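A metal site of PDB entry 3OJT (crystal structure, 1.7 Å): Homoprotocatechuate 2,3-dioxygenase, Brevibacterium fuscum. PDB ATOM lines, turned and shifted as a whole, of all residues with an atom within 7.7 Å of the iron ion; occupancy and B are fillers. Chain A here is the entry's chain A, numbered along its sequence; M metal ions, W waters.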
ATOM      1  N   ASP A 154      36.039  17.165  -0.148  1.00  0.00           N
ATOM      2  CA  ASP A 154      35.442  15.863  -0.405  1.00  0.00           C
ATOM      3  C   ASP A 154      34.447  15.855  -1.560  1.00  0.00           C
ATOM      4  O   ASP A 154      34.541  14.994  -2.427  1.00  0.00           O
ATOM      5  CB  ASP A 154      34.755  15.242   0.800  1.00  0.00           C
ATOM      6  CG  ASP A 154      34.361  13.744   0.534  1.00  0.00           C
ATOM      7  OD1 ASP A 154      35.275  12.859   0.643  1.00  0.00           O
ATOM      8  OD2 ASP A 154      33.169  13.452   0.213  1.00  0.00           O
ATOM      9  N   HIS A 155      33.465  16.747  -1.518  1.00  0.00           N
ATOM     10  CA  HIS A 155      32.432  16.765  -2.569  1.00  0.00           C
ATOM     11  C   HIS A 155      31.698  18.072  -2.705  1.00  0.00           C
ATOM     12  O   HIS A 155      31.791  18.928  -1.839  1.00  0.00           O
ATOM     13  CB  HIS A 155      31.414  15.658  -2.283  1.00  0.00           C
ATOM     14  CG  HIS A 155      30.640  15.804  -1.012  1.00  0.00           C
ATOM     15  ND1 HIS A 155      31.006  15.191   0.165  1.00  0.00           N
ATOM     16  CD2 HIS A 155      29.464  16.441  -0.741  1.00  0.00           C
ATOM     17  CE1 HIS A 155      30.099  15.437   1.104  1.00  0.00           C
ATOM     18  NE2 HIS A 155      29.136  16.187   0.570  1.00  0.00           N
ATOM     19  N   PHE A 156      30.933  18.172  -3.800  1.00  0.00           N
ATOM     20  CA  PHE A 156      29.942  19.198  -4.017  1.00  0.00           C
ATOM     21  C   PHE A 156      28.533  18.530  -3.929  1.00  0.00           C
ATOM     22  O   PHE A 156      28.388  17.314  -4.070  1.00  0.00           O
ATOM     23  CB  PHE A 156      30.063  19.778  -5.443  1.00  0.00           C
ATOM     24  CG  PHE A 156      31.462  20.217  -5.827  1.00  0.00           C
ATOM     25  CD1 PHE A 156      32.180  21.072  -5.009  1.00  0.00           C
ATOM     26  CD2 PHE A 156      32.034  19.792  -7.016  1.00  0.00           C
ATOM     27  CE1 PHE A 156      33.483  21.503  -5.375  1.00  0.00           C
ATOM     28  CE2 PHE A 156      33.321  20.180  -7.377  1.00  0.00           C
ATOM     29  CZ  PHE A 156      34.044  21.046  -6.551  1.00  0.00           C
ATOM     30  N   ASN A 157      27.516  19.319  -3.674  1.00  0.00           N
ATOM     31  CA  ASN A 157      26.172  18.776  -3.716  1.00  0.00           C
ATOM     32  C   ASN A 157      25.319  19.826  -4.414  1.00  0.00           C
ATOM     33  O   ASN A 157      25.307  20.967  -4.012  1.00  0.00           O
ATOM     34  CB  ASN A 157      25.666  18.481  -2.303  1.00  0.00           C
ATOM     35  CG  ASN A 157      24.306  17.855  -2.293  1.00  0.00           C
ATOM     36  OD1 ASN A 157      23.365  18.421  -2.835  1.00  0.00           O
ATOM     37  ND2 ASN A 157      24.184  16.678  -1.652  1.00  0.00           N
ATOM     38  N   TRP A 192      23.842  10.089  -5.216  1.00  0.00           N
ATOM     39  CA  TRP A 192      25.230  10.368  -4.876  1.00  0.00           C
ATOM     40  C   TRP A 192      26.101   9.657  -5.892  1.00  0.00           C
ATOM     41  O   TRP A 192      25.867   8.498  -6.168  1.00  0.00           O
ATOM     42  CB  TRP A 192      25.531   9.817  -3.456  1.00  0.00           C
ATOM     43  CG  TRP A 192      25.001  10.636  -2.329  1.00  0.00           C
ATOM     44  CD1 TRP A 192      25.741  11.437  -1.485  1.00  0.00           C
ATOM     45  CD2 TRP A 192      23.659  10.702  -1.846  1.00  0.00           C
ATOM     46  NE1 TRP A 192      24.931  12.007  -0.524  1.00  0.00           N
ATOM     47  CE2 TRP A 192      23.638  11.598  -0.744  1.00  0.00           C
ATOM     48  CE3 TRP A 192      22.464  10.093  -2.243  1.00  0.00           C
ATOM     49  CZ2 TRP A 192      22.459  11.905  -0.036  1.00  0.00           C
ATOM     50  CZ3 TRP A 192      21.280  10.432  -1.567  1.00  0.00           C
ATOM     51  CH2 TRP A 192      21.290  11.307  -0.465  1.00  0.00           C
ATOM     52  N   HIS A 200      31.065   9.936  -2.761  1.00  0.00           N
ATOM     53  CA  HIS A 200      30.791  10.858  -3.836  1.00  0.00           C
ATOM     54  C   HIS A 200      31.797  11.973  -4.046  1.00  0.00           C
ATOM     55  O   HIS A 200      32.553  12.309  -3.151  1.00  0.00           O
ATOM     56  CB  HIS A 200      29.382  11.466  -3.755  1.00  0.00           C
ATOM     57  CG  HIS A 200      29.059  12.184  -2.483  1.00  0.00           C
ATOM     58  ND1 HIS A 200      29.452  11.750  -1.228  1.00  0.00           N
ATOM     59  CD2 HIS A 200      28.290  13.279  -2.272  1.00  0.00           C
ATOM     60  CE1 HIS A 200      28.950  12.572  -0.308  1.00  0.00           C
ATOM     61  NE2 HIS A 200      28.228  13.492  -0.921  1.00  0.00           N
ATOM     62  N   ALA A 203      26.755  15.217  -5.801  1.00  0.00           N
ATOM     63  CA  ALA A 203      25.461  14.646  -5.473  1.00  0.00           C
ATOM     64  C   ALA A 203      24.418  15.564  -6.046  1.00  0.00           C
ATOM     65  O   ALA A 203      24.639  16.761  -6.204  1.00  0.00           O
ATOM     66  CB  ALA A 203      25.282  14.552  -3.957  1.00  0.00           C
ATOM     67  N   THR A 205      20.512  16.795  -5.411  1.00  0.00           N
ATOM     68  CA  THR A 205      19.422  16.934  -4.456  1.00  0.00           C
ATOM     69  C   THR A 205      18.249  17.545  -5.216  1.00  0.00           C
ATOM     70  O   THR A 205      18.380  18.581  -5.895  1.00  0.00           O
ATOM     71  CB  THR A 205      19.814  17.804  -3.248  1.00  0.00           C
ATOM     72  OG1 THR A 205      20.976  17.236  -2.611  1.00  0.00           O
ATOM     73  CG2 THR A 205      18.635  17.958  -2.273  1.00  0.00           C
ATOM     74  N   HIS A 213      23.962  23.280  -3.167  1.00  0.00           N
ATOM     75  CA  HIS A 213      23.520  23.038  -1.833  1.00  0.00           C
ATOM     76  C   HIS A 213      24.664  23.284  -0.841  1.00  0.00           C
ATOM     77  O   HIS A 213      24.499  23.980   0.152  1.00  0.00           O
ATOM     78  CB  HIS A 213      22.976  21.616  -1.678  1.00  0.00           C
ATOM     79  CG  HIS A 213      22.157  21.467  -0.450  1.00  0.00           C
ATOM     80  ND1 HIS A 213      22.703  21.209   0.786  1.00  0.00           N
ATOM     81  CD2 HIS A 213      20.815  21.607  -0.249  1.00  0.00           C
ATOM     82  CE1 HIS A 213      21.747  21.182   1.692  1.00  0.00           C
ATOM     83  NE2 HIS A 213      20.587  21.425   1.094  1.00  0.00           N
ATOM     84  N   HIS A 214      25.801  22.636  -1.084  1.00  0.00           N
ATOM     85  CA  HIS A 214      26.976  22.842  -0.240  1.00  0.00           C
ATOM     86  C   HIS A 214      28.246  22.358  -0.875  1.00  0.00           C
ATOM     87  O   HIS A 214      28.229  21.705  -1.887  1.00  0.00           O
ATOM     88  CB  HIS A 214      26.804  22.143   1.126  1.00  0.00           C
ATOM     89  CG  HIS A 214      26.549  20.675   1.039  1.00  0.00           C
ATOM     90  ND1 HIS A 214      25.281  20.152   1.012  1.00  0.00           N
ATOM     91  CD2 HIS A 214      27.392  19.612   1.042  1.00  0.00           C
ATOM     92  CE1 HIS A 214      25.349  18.832   0.936  1.00  0.00           C
ATOM     93  NE2 HIS A 214      26.621  18.492   0.967  1.00  0.00           N
ATOM     94  N   VAL A 215      29.350  22.731  -0.246  1.00  0.00           N
ATOM     95  CA  VAL A 215      30.682  22.217  -0.542  1.00  0.00           C
ATOM     96  C   VAL A 215      31.110  21.497   0.742  1.00  0.00           C
ATOM     97  O   VAL A 215      30.857  22.014   1.828  1.00  0.00           O
ATOM     98  CB  VAL A 215      31.647  23.400  -0.852  1.00  0.00           C
ATOM     99  CG1 VAL A 215      33.092  22.952  -0.794  1.00  0.00           C
ATOM    100  CG2 VAL A 215      31.301  24.059  -2.216  1.00  0.00           C
ATOM    101  N   ALA A 216      31.723  20.320   0.641  1.00  0.00           N
ATOM    102  CA  ALA A 216      32.065  19.535   1.833  1.00  0.00           C
ATOM    103  C   ALA A 216      33.566  19.370   1.946  1.00  0.00           C
ATOM    104  O   ALA A 216      34.233  19.075   0.947  1.00  0.00           O
ATOM    105  CB  ALA A 216      31.393  18.159   1.770  1.00  0.00           C
ATOM    106  N   HIS A 248      25.323  10.375   9.098  1.00  0.00           N
ATOM    107  CA  HIS A 248      24.451  10.159   7.948  1.00  0.00           C
ATOM    108  C   HIS A 248      24.025   8.688   7.836  1.00  0.00           C
ATOM    109  O   HIS A 248      24.803   7.761   8.184  1.00  0.00           O
ATOM    110  CB  HIS A 248      25.128  10.529   6.640  1.00  0.00           C
ATOM    111  CG  HIS A 248      25.222  12.005   6.375  1.00  0.00           C
ATOM    112  ND1 HIS A 248      24.118  12.834   6.384  1.00  0.00           N
ATOM    113  CD2 HIS A 248      26.291  12.778   6.031  1.00  0.00           C
ATOM    114  CE1 HIS A 248      24.504  14.069   6.096  1.00  0.00           C
ATOM    115  NE2 HIS A 248      25.813  14.058   5.871  1.00  0.00           N
ATOM    116  N   SER A 251      25.723   7.350   2.985  1.00  0.00           N
ATOM    117  CA  SER A 251      27.179   7.673   3.084  1.00  0.00           C
ATOM    118  C   SER A 251      27.833   7.150   4.352  1.00  0.00           C
ATOM    119  O   SER A 251      29.022   6.954   4.356  1.00  0.00           O
ATOM    120  CB  SER A 251      27.548   9.158   2.890  1.00  0.00           C
ATOM    121  OG  SER A 251      27.400   9.907   4.089  1.00  0.00           O
ATOM    122  N   TYR A 255      29.033  14.047  10.272  1.00  0.00           N
ATOM    123  CA  TYR A 255      28.830  15.321   9.566  1.00  0.00           C
ATOM    124  C   TYR A 255      28.424  16.488  10.423  1.00  0.00           C
ATOM    125  O   TYR A 255      27.921  16.338  11.540  1.00  0.00           O
ATOM    126  CB  TYR A 255      27.752  15.168   8.463  1.00  0.00           C
ATOM    127  CG  TYR A 255      26.335  15.079   8.981  1.00  0.00           C
ATOM    128  CD1 TYR A 255      25.775  13.839   9.316  1.00  0.00           C
ATOM    129  CD2 TYR A 255      25.572  16.213   9.172  1.00  0.00           C
ATOM    130  CE1 TYR A 255      24.438  13.746   9.818  1.00  0.00           C
ATOM    131  CE2 TYR A 255      24.257  16.142   9.694  1.00  0.00           C
ATOM    132  CZ  TYR A 255      23.711  14.899  10.011  1.00  0.00           C
ATOM    133  OH  TYR A 255      22.401  14.847  10.476  1.00  0.00           O
ATOM    134  N   TYR A 257      26.783  20.660   9.272  1.00  0.00           N
ATOM    135  CA  TYR A 257      26.527  21.745   8.304  1.00  0.00           C
ATOM    136  C   TYR A 257      26.520  23.104   8.995  1.00  0.00           C
ATOM    137  O   TYR A 257      25.809  23.296   9.999  1.00  0.00           O
ATOM    138  CB  TYR A 257      25.171  21.556   7.613  1.00  0.00           C
ATOM    139  CG  TYR A 257      25.045  20.281   6.826  1.00  0.00           C
ATOM    140  CD1 TYR A 257      25.470  20.200   5.498  1.00  0.00           C
ATOM    141  CD2 TYR A 257      24.481  19.153   7.397  1.00  0.00           C
ATOM    142  CE1 TYR A 257      25.366  19.035   4.790  1.00  0.00           C
ATOM    143  CE2 TYR A 257      24.366  17.953   6.681  1.00  0.00           C
ATOM    144  CZ  TYR A 257      24.813  17.898   5.395  1.00  0.00           C
ATOM    145  OH  TYR A 257      24.674  16.742   4.681  1.00  0.00           O
ATOM    146  N   GLU A 267      29.680  21.759   4.527  1.00  0.00           N
ATOM    147  CA  GLU A 267      29.608  20.507   5.288  1.00  0.00           C
ATOM    148  C   GLU A 267      31.025  20.082   5.745  1.00  0.00           C
ATOM    149  O   GLU A 267      31.963  20.162   4.971  1.00  0.00           O
ATOM    150  CB  GLU A 267      29.031  19.386   4.430  1.00  0.00           C
ATOM    151  CG  GLU A 267      28.639  18.181   5.265  1.00  0.00           C
ATOM    152  CD  GLU A 267      28.184  16.996   4.427  1.00  0.00           C
ATOM    153  OE1 GLU A 267      28.113  17.160   3.213  1.00  0.00           O
ATOM    154  OE2 GLU A 267      27.942  15.903   4.977  1.00  0.00           O
ATOM    155  N   ILE A 268      31.144  19.631   6.993  1.00  0.00           N
ATOM    156  CA  ILE A 268      32.326  18.942   7.476  1.00  0.00           C
ATOM    157  C   ILE A 268      31.930  17.467   7.618  1.00  0.00           C
ATOM    158  O   ILE A 268      30.852  17.175   8.122  1.00  0.00           O
ATOM    159  CB  ILE A 268      32.885  19.492   8.829  1.00  0.00           C
ATOM    160  CG1 ILE A 268      32.690  21.002   8.956  1.00  0.00           C
ATOM    161  CG2 ILE A 268      34.368  19.035   9.038  1.00  0.00           C
ATOM    162  CD1 ILE A 268      33.327  21.798   7.924  1.00  0.00           C
ATOM    163  N   TYR A 269      32.773  16.590   7.119  1.00  0.00           N
ATOM    164  CA  TYR A 269      32.447  15.204   6.779  1.00  0.00           C
ATOM    165  C   TYR A 269      33.642  14.284   7.156  1.00  0.00           C
ATOM    166  O   TYR A 269      34.795  14.656   7.008  1.00  0.00           O
ATOM    167  CB  TYR A 269      32.155  15.249   5.262  1.00  0.00           C
ATOM    168  CG  TYR A 269      31.729  14.026   4.516  1.00  0.00           C
ATOM    169  CD1 TYR A 269      30.395  13.706   4.364  1.00  0.00           C
ATOM    170  CD2 TYR A 269      32.669  13.217   3.883  1.00  0.00           C
ATOM    171  CE1 TYR A 269      29.979  12.611   3.623  1.00  0.00           C
ATOM    172  CE2 TYR A 269      32.266  12.123   3.146  1.00  0.00           C
ATOM    173  CZ  TYR A 269      30.915  11.827   3.022  1.00  0.00           C
ATOM    174  OH  TYR A 269      30.521  10.765   2.257  1.00  0.00           O
ATOM    175  N   ARG A 293      18.876  10.239   6.463  1.00  0.00           N
ATOM    176  CA  ARG A 293      19.688  11.433   6.415  1.00  0.00           C
ATOM    177  C   ARG A 293      20.445  11.632   7.700  1.00  0.00           C
ATOM    178  O   ARG A 293      21.596  11.940   7.648  1.00  0.00           O
ATOM    179  CB  ARG A 293      18.846  12.676   6.119  1.00  0.00           C
ATOM    180  CG  ARG A 293      18.428  12.694   4.667  1.00  0.00           C
ATOM    181  CD  ARG A 293      18.109  14.080   4.132  1.00  0.00           C
ATOM    182  NE  ARG A 293      17.802  14.058   2.684  1.00  0.00           N
ATOM    183  CZ  ARG A 293      18.692  14.092   1.690  1.00  0.00           C
ATOM    184  NH1 ARG A 293      19.992  14.166   1.932  1.00  0.00           N
ATOM    185  NH2 ARG A 293      18.279  14.081   0.437  1.00  0.00           N
ATOM    186  N   TRP A 304      17.361  23.410   5.576  1.00  0.00           N
ATOM    187  CA  TRP A 304      18.301  22.536   4.906  1.00  0.00           C
ATOM    188  C   TRP A 304      17.738  22.117   3.575  1.00  0.00           C
ATOM    189  O   TRP A 304      18.483  21.934   2.602  1.00  0.00           O
ATOM    190  CB  TRP A 304      18.637  21.327   5.781  1.00  0.00           C
ATOM    191  CG  TRP A 304      19.856  20.599   5.312  1.00  0.00           C
ATOM    192  CD1 TRP A 304      21.141  20.846   5.668  1.00  0.00           C
ATOM    193  CD2 TRP A 304      19.897  19.531   4.398  1.00  0.00           C
ATOM    194  NE1 TRP A 304      21.993  19.959   5.058  1.00  0.00           N
ATOM    195  CE2 TRP A 304      21.241  19.147   4.251  1.00  0.00           C
ATOM    196  CE3 TRP A 304      18.915  18.848   3.699  1.00  0.00           C
ATOM    197  CZ2 TRP A 304      21.644  18.137   3.389  1.00  0.00           C
ATOM    198  CZ3 TRP A 304      19.320  17.824   2.858  1.00  0.00           C
ATOM    199  CH2 TRP A 304      20.678  17.456   2.731  1.00  0.00           C
HETATM  200 FE    FE M   1      27.195  16.386   1.530  1.00  0.00          FE
HETATM  201  O   HOH W   1      25.189  16.116   2.476  1.00  0.00           O
HETATM  202  O   HOH W   2      26.349  15.371  -0.148  1.00  0.00           O
HETATM  203  O   HOH W   3      27.471  14.367   2.572  1.00  0.00           O
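His 200 touches the iron ion. Of the 21 residues printed, 4 come within 4 Å of the iron ion.
ND1 of His 214 is in hydrogen-bond range of ND1 of His 213 (2.8 Å). The side-chain carboxylate (OE2) of Glu 267 lies within hydrogen-bond range of a ring nitrogen (NE2) of His 248 (3.0 Å). ND1 of His 155 sits at hydrogen-bond distance from OD2 of Asp 154. The backbone carbonyl oxygen (O) of Val 215 is in hydrogen-bond range of the backbone NH (N) of Glu 267 (3.0 Å). The backbone carbonyl oxygen of His 214 lies within hydrogen-bond range of the backbone NH of Asn 157, 3.1 Å away. The side-chain carboxylate of Glu 267 sits at hydrogen-bond distance from the side-chain hydroxyl of Tyr 257 (3.4 Å). The backbone NH of Ala 216 lies within hydrogen-bond range of the backbone carbonyl oxygen of His 155 (2.8 Å). ND1 of His 155 lies close to NE2 of His 200, 3.4 Å away.
Water W2 bridges NE2 of His 200 (2.8 Å) and ND2 of Asn 157 (2.9 Å).
The iron ion is bound by the side-chain carboxylate of Glu 267 (2.1 Å), water W2 (2.1 Å), a ring nitrogen (NE2) of His 155 (2.2 Å), water W1 (2.2 Å), a ring nitrogen (NE2) of His 214 (2.3 Å) and water W3 (2.3 Å). The iron ion has six donor atoms within binding distance.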
